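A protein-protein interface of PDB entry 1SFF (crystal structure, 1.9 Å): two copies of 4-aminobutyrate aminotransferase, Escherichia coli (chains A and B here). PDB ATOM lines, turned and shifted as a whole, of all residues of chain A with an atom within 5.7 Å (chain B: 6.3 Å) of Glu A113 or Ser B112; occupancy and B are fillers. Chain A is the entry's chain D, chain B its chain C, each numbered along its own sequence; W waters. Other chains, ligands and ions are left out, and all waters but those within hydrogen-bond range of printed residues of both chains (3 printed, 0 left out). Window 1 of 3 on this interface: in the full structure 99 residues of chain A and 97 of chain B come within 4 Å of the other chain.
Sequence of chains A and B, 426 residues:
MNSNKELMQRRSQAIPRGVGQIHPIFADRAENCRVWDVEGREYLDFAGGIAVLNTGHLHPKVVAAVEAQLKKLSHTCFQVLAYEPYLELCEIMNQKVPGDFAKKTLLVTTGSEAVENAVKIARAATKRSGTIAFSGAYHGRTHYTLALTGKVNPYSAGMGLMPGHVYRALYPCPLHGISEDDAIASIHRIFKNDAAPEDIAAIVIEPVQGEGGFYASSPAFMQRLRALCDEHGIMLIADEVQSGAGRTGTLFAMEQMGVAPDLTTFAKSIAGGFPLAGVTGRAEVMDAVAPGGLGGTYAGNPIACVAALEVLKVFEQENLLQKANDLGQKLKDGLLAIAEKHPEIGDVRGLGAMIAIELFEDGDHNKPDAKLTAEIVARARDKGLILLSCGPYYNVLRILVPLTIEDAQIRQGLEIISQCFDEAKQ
The side-chain hydroxyl of Thr B110 lies within hydrogen-bond range of the side-chain carboxylate of Glu A113 (3.1 Å).
The side-chain hydroxyl (OG) of Ser B112 sits at hydrogen-bond distance from the side-chain carboxylate (OE2) of Glu A113, 3.3 Å away.
The side-chain hydroxyl of Thr A110 is in hydrogen-bond range of the side-chain carboxylate of Glu B113, at 3.1 Å.
The side-chain carboxylate (OE2) of Glu B113 lies within hydrogen-bond range of the side-chain hydroxyl (OG) of Ser A112 (3.4 Å).
The side-chain hydroxyl (OG1) of Thr B110 sits at hydrogen-bond distance from the backbone NH (N) of Glu B113.
The side-chain hydroxyl (OG1) of Thr B142 sits at hydrogen-bond distance from the side-chain carboxylate (OE2) of Glu B116 (2.5 Å).
The side-chain hydroxyl (OG1) of Thr B142 sits at hydrogen-bond distance from the side-chain hydroxyl (OG1) of Thr B145 (2.7 Å).
The backbone NH (N) of Thr A109 is in hydrogen-bond range of the side-chain carboxylate (OE1) of Glu A113 (3.0 Å).
OG1 of Thr A110 lies within hydrogen-bond range of N of Glu A113, 3.2 Å away.
OD1 of Asn A117 sits close to O of Glu A113.
Thr A109 touches Thr B110.
CD of Glu A116 touches CB of Thr B142, 3.6 Å away.
CB of Thr A142 touches OE2 of Glu B116 (3.6 Å).
Of the printed residues of chain B, Glu A116 touches Thr B142.
Of the printed residues of chain A, Ser B112 touches Glu A113.
Of the printed residues of chain A, Glu B116 touches Thr A142.
Arg B141 touches none of the printed residues of chain A.
Of the printed residues of chain A, Thr B142 touches Glu A116.
Of the 13 printed residues of chain A, 6 touch a printed residue of chain B.
Printed residues of chain A that touch a printed residue of chain B: Thr A109, Thr A110, Ser A112, Glu A113, Glu A116 and Thr A142.
Along chain B the printed residues that touch a printed residue of chain A span positions 110 to 142.
Among the printed residues, no Asp or Glu carboxylate lies within 4 Å of a Lys or Arg side-chain nitrogen of the other chain.
Thr A110 touches Glu B113, and with the chains exchanged Glu A113 touches Thr B110.
Ser A112 touches Glu B113, and with the chains exchanged Glu A113 touches Ser B112.
Glu A116 touches Thr B142, and with the chains exchanged Thr A142 touches Glu B116.
9 positions are printed for both chains.
Of the 7 pairs that touch across the chains among the printed residues, 6 have their exchanged pair printed and touching as well.
Water W3 bridges OE2 of Glu B116 (2.7 Å) and OE2 of Glu A116 (2.7 Å).
Water W2 bridges OE2 of Glu A113 and OG of Ser B112.
Water W1 bridges the side-chain carboxylate (OE2) of Glu B113 (2.8 Å) and the side-chain hydroxyl (OG) of Ser A112 (3.0 Å).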
ATOM      1  N   VAL A 108      26.598  14.667  11.788  1.00  0.00           N
ATOM      2  CA  VAL A 108      26.999  15.048  10.436  1.00  0.00           C
ATOM      3  C   VAL A 108      27.631  16.463  10.585  1.00  0.00           C
ATOM      4  O   VAL A 108      28.286  16.748  11.608  1.00  0.00           O
ATOM      5  CB  VAL A 108      25.819  15.056   9.405  1.00  0.00           C
ATOM      6  CG1 VAL A 108      25.461  13.594   9.066  1.00  0.00           C
ATOM      7  CG2 VAL A 108      24.577  15.840   9.963  1.00  0.00           C
ATOM      8  N   THR A 109      27.428  17.357   9.623  1.00  0.00           N
ATOM      9  CA  THR A 109      28.070  18.679   9.736  1.00  0.00           C
ATOM     10  C   THR A 109      27.114  19.855   9.606  1.00  0.00           C
ATOM     11  O   THR A 109      27.247  20.804  10.354  1.00  0.00           O
ATOM     12  CB  THR A 109      29.185  18.808   8.671  1.00  0.00           C
ATOM     13  OG1 THR A 109      30.069  17.710   8.844  1.00  0.00           O
ATOM     14  CG2 THR A 109      29.991  20.169   8.784  1.00  0.00           C
ATOM     15  N   THR A 110      26.157  19.809   8.667  1.00  0.00           N
ATOM     16  CA  THR A 110      25.247  20.935   8.545  1.00  0.00           C
ATOM     17  C   THR A 110      23.808  20.592   8.873  1.00  0.00           C
ATOM     18  O   THR A 110      23.419  19.430   8.846  1.00  0.00           O
ATOM     19  CB  THR A 110      25.288  21.532   7.111  1.00  0.00           C
ATOM     20  OG1 THR A 110      24.617  20.641   6.201  1.00  0.00           O
ATOM     21  CG2 THR A 110      26.733  21.759   6.690  1.00  0.00           C
ATOM     22  N   GLY A 111      23.021  21.607   9.208  1.00  0.00           N
ATOM     23  CA  GLY A 111      21.613  21.356   9.497  1.00  0.00           C
ATOM     24  C   GLY A 111      20.861  20.720   8.315  1.00  0.00           C
ATOM     25  O   GLY A 111      19.979  19.864   8.521  1.00  0.00           O
ATOM     26  N   SER A 112      21.172  21.127   7.080  1.00  0.00           N
ATOM     27  CA  SER A 112      20.476  20.517   5.948  1.00  0.00           C
ATOM     28  C   SER A 112      20.844  19.028   5.884  1.00  0.00           C
ATOM     29  O   SER A 112      20.002  18.201   5.550  1.00  0.00           O
ATOM     30  CB  SER A 112      20.838  21.201   4.622  1.00  0.00           C
ATOM     31  OG  SER A 112      22.218  21.110   4.366  1.00  0.00           O
ATOM     32  N   GLU A 113      22.105  18.696   6.161  1.00  0.00           N
ATOM     33  CA  GLU A 113      22.505  17.271   6.178  1.00  0.00           C
ATOM     34  C   GLU A 113      21.754  16.530   7.320  1.00  0.00           C
ATOM     35  O   GLU A 113      21.395  15.361   7.177  1.00  0.00           O
ATOM     36  CB  GLU A 113      24.011  17.104   6.425  1.00  0.00           C
ATOM     37  CG  GLU A 113      24.881  17.423   5.249  1.00  0.00           C
ATOM     38  CD  GLU A 113      26.355  17.096   5.534  1.00  0.00           C
ATOM     39  OE1 GLU A 113      26.795  17.287   6.700  1.00  0.00           O
ATOM     40  OE2 GLU A 113      27.068  16.681   4.578  1.00  0.00           O
ATOM     41  N   ALA A 114      21.525  17.194   8.442  1.00  0.00           N
ATOM     42  CA  ALA A 114      20.805  16.533   9.533  1.00  0.00           C
ATOM     43  C   ALA A 114      19.380  16.205   9.055  1.00  0.00           C
ATOM     44  O   ALA A 114      18.916  15.085   9.219  1.00  0.00           O
ATOM     45  CB  ALA A 114      20.767  17.442  10.772  1.00  0.00           C
ATOM     46  N   VAL A 115      18.684  17.172   8.452  1.00  0.00           N
ATOM     47  CA  VAL A 115      17.326  16.895   7.971  1.00  0.00           C
ATOM     48  C   VAL A 115      17.369  15.804   6.878  1.00  0.00           C
ATOM     49  O   VAL A 115      16.549  14.871   6.880  1.00  0.00           O
ATOM     50  CB  VAL A 115      16.647  18.193   7.429  1.00  0.00           C
ATOM     51  CG1 VAL A 115      15.216  17.901   6.900  1.00  0.00           C
ATOM     52  CG2 VAL A 115      16.600  19.197   8.575  1.00  0.00           C
ATOM     53  N   GLU A 116      18.338  15.886   5.967  1.00  0.00           N
ATOM     54  CA  GLU A 116      18.453  14.869   4.914  1.00  0.00           C
ATOM     55  C   GLU A 116      18.540  13.461   5.521  1.00  0.00           C
ATOM     56  O   GLU A 116      17.870  12.527   5.080  1.00  0.00           O
ATOM     57  CB  GLU A 116      19.726  15.088   4.095  1.00  0.00           C
ATOM     58  CG  GLU A 116      19.625  16.286   3.129  1.00  0.00           C
ATOM     59  CD  GLU A 116      19.085  15.882   1.759  1.00  0.00           C
ATOM     60  OE1 GLU A 116      18.808  14.672   1.566  1.00  0.00           O
ATOM     61  OE2 GLU A 116      18.958  16.772   0.869  1.00  0.00           O
ATOM     62  N   ASN A 117      19.397  13.314   6.513  1.00  0.00           N
ATOM     63  CA  ASN A 117      19.562  11.997   7.130  1.00  0.00           C
ATOM     64  C   ASN A 117      18.384  11.559   7.957  1.00  0.00           C
ATOM     65  O   ASN A 117      18.075  10.365   7.997  1.00  0.00           O
ATOM     66  CB  ASN A 117      20.850  11.963   7.952  1.00  0.00           C
ATOM     67  CG  ASN A 117      22.080  11.864   7.050  1.00  0.00           C
ATOM     68  OD1 ASN A 117      22.724  12.877   6.692  1.00  0.00           O
ATOM     69  ND2 ASN A 117      22.390  10.655   6.646  1.00  0.00           N
ATOM     70  N   ALA A 118      17.722  12.485   8.622  1.00  0.00           N
ATOM     71  CA  ALA A 118      16.537  12.096   9.410  1.00  0.00           C
ATOM     72  C   ALA A 118      15.476  11.522   8.469  1.00  0.00           C
ATOM     73  O   ALA A 118      14.805  10.531   8.788  1.00  0.00           O
ATOM     74  CB  ALA A 118      15.977  13.328  10.194  1.00  0.00           C
ATOM     75  N   THR A 142      19.667  21.959   0.272  1.00  0.00           N
ATOM     76  CA  THR A 142      20.011  20.897  -0.641  1.00  0.00           C
ATOM     77  C   THR A 142      18.720  20.691  -1.439  1.00  0.00           C
ATOM     78  O   THR A 142      17.660  21.171  -1.029  1.00  0.00           O
ATOM     79  CB  THR A 142      20.358  19.580   0.097  1.00  0.00           C
ATOM     80  OG1 THR A 142      19.259  19.221   0.962  1.00  0.00           O
ATOM     81  CG2 THR A 142      21.616  19.771   0.929  1.00  0.00           C
ATOM     82  N   VAL A 279      21.515  13.999  14.238  1.00  0.00           N
ATOM     83  CA  VAL A 279      20.158  13.484  14.297  1.00  0.00           C
ATOM     84  C   VAL A 279      20.107  12.523  15.501  1.00  0.00           C
ATOM     85  O   VAL A 279      20.933  11.621  15.574  1.00  0.00           O
ATOM     86  CB  VAL A 279      19.805  12.650  13.047  1.00  0.00           C
ATOM     87  CG1 VAL A 279      18.361  12.121  13.225  1.00  0.00           C
ATOM     88  CG2 VAL A 279      19.938  13.500  11.733  1.00  0.00           C
ATOM     89  N   THR B 110      30.332  21.052   3.150  1.00  0.00           N
ATOM     90  CA  THR B 110      30.687  19.653   2.789  1.00  0.00           C
ATOM     91  C   THR B 110      30.746  19.406   1.276  1.00  0.00           C
ATOM     92  O   THR B 110      30.160  20.166   0.492  1.00  0.00           O
ATOM     93  CB  THR B 110      29.659  18.635   3.399  1.00  0.00           C
ATOM     94  OG1 THR B 110      28.386  18.779   2.758  1.00  0.00           O
ATOM     95  CG2 THR B 110      29.484  18.935   4.895  1.00  0.00           C
ATOM     96  N   GLY B 111      31.461  18.358   0.886  1.00  0.00           N
ATOM     97  CA  GLY B 111      31.558  18.017  -0.519  1.00  0.00           C
ATOM     98  C   GLY B 111      30.162  17.743  -1.097  1.00  0.00           C
ATOM     99  O   GLY B 111      29.921  18.085  -2.250  1.00  0.00           O
ATOM    100  N   SER B 112      29.249  17.131  -0.334  1.00  0.00           N
ATOM    101  CA  SER B 112      27.918  16.873  -0.893  1.00  0.00           C
ATOM    102  C   SER B 112      27.191  18.195  -1.125  1.00  0.00           C
ATOM    103  O   SER B 112      26.478  18.341  -2.108  1.00  0.00           O
ATOM    104  CB  SER B 112      27.070  15.963   0.016  1.00  0.00           C
ATOM    105  OG  SER B 112      26.812  16.556   1.265  1.00  0.00           O
ATOM    106  N   GLU B 113      27.355  19.150  -0.212  1.00  0.00           N
ATOM    107  CA  GLU B 113      26.733  20.458  -0.433  1.00  0.00           C
ATOM    108  C   GLU B 113      27.359  21.162  -1.654  1.00  0.00           C
ATOM    109  O   GLU B 113      26.689  21.935  -2.349  1.00  0.00           O
ATOM    110  CB  GLU B 113      26.920  21.378   0.772  1.00  0.00           C
ATOM    111  CG  GLU B 113      26.053  21.047   1.954  1.00  0.00           C
ATOM    112  CD  GLU B 113      26.223  22.106   3.033  1.00  0.00           C
ATOM    113  OE1 GLU B 113      27.357  22.618   3.158  1.00  0.00           O
ATOM    114  OE2 GLU B 113      25.244  22.416   3.743  1.00  0.00           O
ATOM    115  N   ALA B 114      28.647  20.948  -1.883  1.00  0.00           N
ATOM    116  CA  ALA B 114      29.284  21.581  -3.045  1.00  0.00           C
ATOM    117  C   ALA B 114      28.618  21.029  -4.324  1.00  0.00           C
ATOM    118  O   ALA B 114      28.222  21.795  -5.215  1.00  0.00           O
ATOM    119  CB  ALA B 114      30.791  21.289  -3.053  1.00  0.00           C
ATOM    120  N   VAL B 115      28.473  19.705  -4.412  1.00  0.00           N
ATOM    121  CA  VAL B 115      27.843  19.124  -5.586  1.00  0.00           C
ATOM    122  C   VAL B 115      26.391  19.577  -5.746  1.00  0.00           C
ATOM    123  O   VAL B 115      25.947  19.850  -6.868  1.00  0.00           O
ATOM    124  CB  VAL B 115      27.894  17.558  -5.592  1.00  0.00           C
ATOM    125  CG1 VAL B 115      27.191  17.006  -6.843  1.00  0.00           C
ATOM    126  CG2 VAL B 115      29.351  17.089  -5.579  1.00  0.00           C
ATOM    127  N   GLU B 116      25.653  19.633  -4.643  1.00  0.00           N
ATOM    128  CA  GLU B 116      24.278  20.097  -4.674  1.00  0.00           C
ATOM    129  C   GLU B 116      24.219  21.521  -5.289  1.00  0.00           C
ATOM    130  O   GLU B 116      23.329  21.850  -6.100  1.00  0.00           O
ATOM    131  CB  GLU B 116      23.739  20.197  -3.247  1.00  0.00           C
ATOM    132  CG  GLU B 116      23.383  18.822  -2.609  1.00  0.00           C
ATOM    133  CD  GLU B 116      21.946  18.422  -2.895  1.00  0.00           C
ATOM    134  OE1 GLU B 116      21.242  19.199  -3.580  1.00  0.00           O
ATOM    135  OE2 GLU B 116      21.506  17.331  -2.420  1.00  0.00           O
ATOM    136  N   ASN B 117      25.137  22.364  -4.837  1.00  0.00           N
ATOM    137  CA  ASN B 117      25.131  23.738  -5.287  1.00  0.00           C
ATOM    138  C   ASN B 117      25.546  23.890  -6.740  1.00  0.00           C
ATOM    139  O   ASN B 117      24.956  24.700  -7.465  1.00  0.00           O
ATOM    140  CB  ASN B 117      25.984  24.589  -4.347  1.00  0.00           C
ATOM    141  CG  ASN B 117      25.224  24.948  -3.092  1.00  0.00           C
ATOM    142  OD1 ASN B 117      25.214  24.204  -2.090  1.00  0.00           O
ATOM    143  ND2 ASN B 117      24.519  26.045  -3.157  1.00  0.00           N
ATOM    144  N   HIS B 139      29.079  10.961  -5.338  1.00  0.00           N
ATOM    145  CA  HIS B 139      28.968  12.417  -5.203  1.00  0.00           C
ATOM    146  C   HIS B 139      28.425  12.906  -3.857  1.00  0.00           C
ATOM    147  O   HIS B 139      28.231  14.120  -3.661  1.00  0.00           O
ATOM    148  CB  HIS B 139      28.107  12.954  -6.363  1.00  0.00           C
ATOM    149  CG  HIS B 139      28.774  12.816  -7.692  1.00  0.00           C
ATOM    150  ND1 HIS B 139      28.309  11.975  -8.683  1.00  0.00           N
ATOM    151  CD2 HIS B 139      29.894  13.395  -8.183  1.00  0.00           C
ATOM    152  CE1 HIS B 139      29.117  12.044  -9.728  1.00  0.00           C
ATOM    153  NE2 HIS B 139      30.089  12.894  -9.448  1.00  0.00           N
ATOM    154  N   GLY B 140      28.191  11.984  -2.914  1.00  0.00           N
ATOM    155  CA  GLY B 140      27.701  12.446  -1.626  1.00  0.00           C
ATOM    156  C   GLY B 140      26.496  11.708  -1.090  1.00  0.00           C
ATOM    157  O   GLY B 140      25.883  10.892  -1.793  1.00  0.00           O
ATOM    158  N   ARG B 141      26.107  12.052   0.135  1.00  0.00           N
ATOM    159  CA  ARG B 141      25.013  11.355   0.787  1.00  0.00           C
ATOM    160  C   ARG B 141      23.700  12.096   1.060  1.00  0.00           C
ATOM    161  O   ARG B 141      22.959  11.698   1.949  1.00  0.00           O
ATOM    162  CB  ARG B 141      25.541  10.756   2.098  1.00  0.00           C
ATOM    163  CG  ARG B 141      26.729   9.746   1.932  1.00  0.00           C
ATOM    164  CD  ARG B 141      27.328   9.433   3.339  1.00  0.00           C
ATOM    165  NE  ARG B 141      28.374   8.410   3.321  1.00  0.00           N
ATOM    166  CZ  ARG B 141      28.149   7.094   3.349  1.00  0.00           C
ATOM    167  NH1 ARG B 141      26.907   6.619   3.400  1.00  0.00           N
ATOM    168  NH2 ARG B 141      29.176   6.245   3.329  1.00  0.00           N
ATOM    169  N   THR B 142      23.405  13.172   0.331  1.00  0.00           N
ATOM    170  CA  THR B 142      22.119  13.823   0.496  1.00  0.00           C
ATOM    171  C   THR B 142      21.227  13.066  -0.537  1.00  0.00           C
ATOM    172  O   THR B 142      21.743  12.335  -1.389  1.00  0.00           O
ATOM    173  CB  THR B 142      22.186  15.304   0.100  1.00  0.00           C
ATOM    174  OG1 THR B 142      22.637  15.397  -1.266  1.00  0.00           O
ATOM    175  CG2 THR B 142      23.183  16.059   1.029  1.00  0.00           C
ATOM    176  N   THR B 145      22.469  13.786  -4.156  1.00  0.00           N
ATOM    177  CA  THR B 145      23.790  13.273  -4.484  1.00  0.00           C
ATOM    178  C   THR B 145      23.842  11.729  -4.427  1.00  0.00           C
ATOM    179  O   THR B 145      24.725  11.100  -5.041  1.00  0.00           O
ATOM    180  CB  THR B 145      24.932  13.935  -3.624  1.00  0.00           C
ATOM    181  OG1 THR B 145      24.632  13.872  -2.227  1.00  0.00           O
ATOM    182  CG2 THR B 145      25.105  15.414  -4.047  1.00  0.00           C
ATOM    183  N   VAL B 241      36.146  17.020  -5.446  1.00  0.00           N
ATOM    184  CA  VAL B 241      36.180  16.910  -4.003  1.00  0.00           C
ATOM    185  C   VAL B 241      37.321  15.991  -3.566  1.00  0.00           C
ATOM    186  O   VAL B 241      38.026  16.304  -2.598  1.00  0.00           O
ATOM    187  CB  VAL B 241      34.826  16.351  -3.499  1.00  0.00           C
ATOM    188  CG1 VAL B 241      34.947  15.785  -2.071  1.00  0.00           C
ATOM    189  CG2 VAL B 241      33.787  17.504  -3.466  1.00  0.00           C
ATOM    190  N   ALA B 267      36.639  20.130  -1.900  1.00  0.00           N
ATOM    191  CA  ALA B 267      36.407  19.989  -0.460  1.00  0.00           C
ATOM    192  C   ALA B 267      37.609  19.193   0.074  1.00  0.00           C
ATOM    193  O   ALA B 267      38.745  19.440  -0.345  1.00  0.00           O
ATOM    194  CB  ALA B 267      35.073  19.237  -0.210  1.00  0.00           C
ATOM    195  N   ALA B 277      34.159  23.404   1.934  1.00  0.00           N
ATOM    196  CA  ALA B 277      33.919  22.916   0.580  1.00  0.00           C
ATOM    197  C   ALA B 277      33.519  24.146  -0.267  1.00  0.00           C
ATOM    198  O   ALA B 277      33.234  25.228   0.274  1.00  0.00           O
ATOM    199  CB  ALA B 277      32.765  21.867   0.566  1.00  0.00           C
HETATM  200  O   HOH W   1      22.955  23.167   2.369  1.00  0.00           O
HETATM  201  O   HOH W   2      26.020  14.656   3.092  1.00  0.00           O
HETATM  202  O   HOH W   3      19.012  16.602  -1.821  1.00  0.00           O
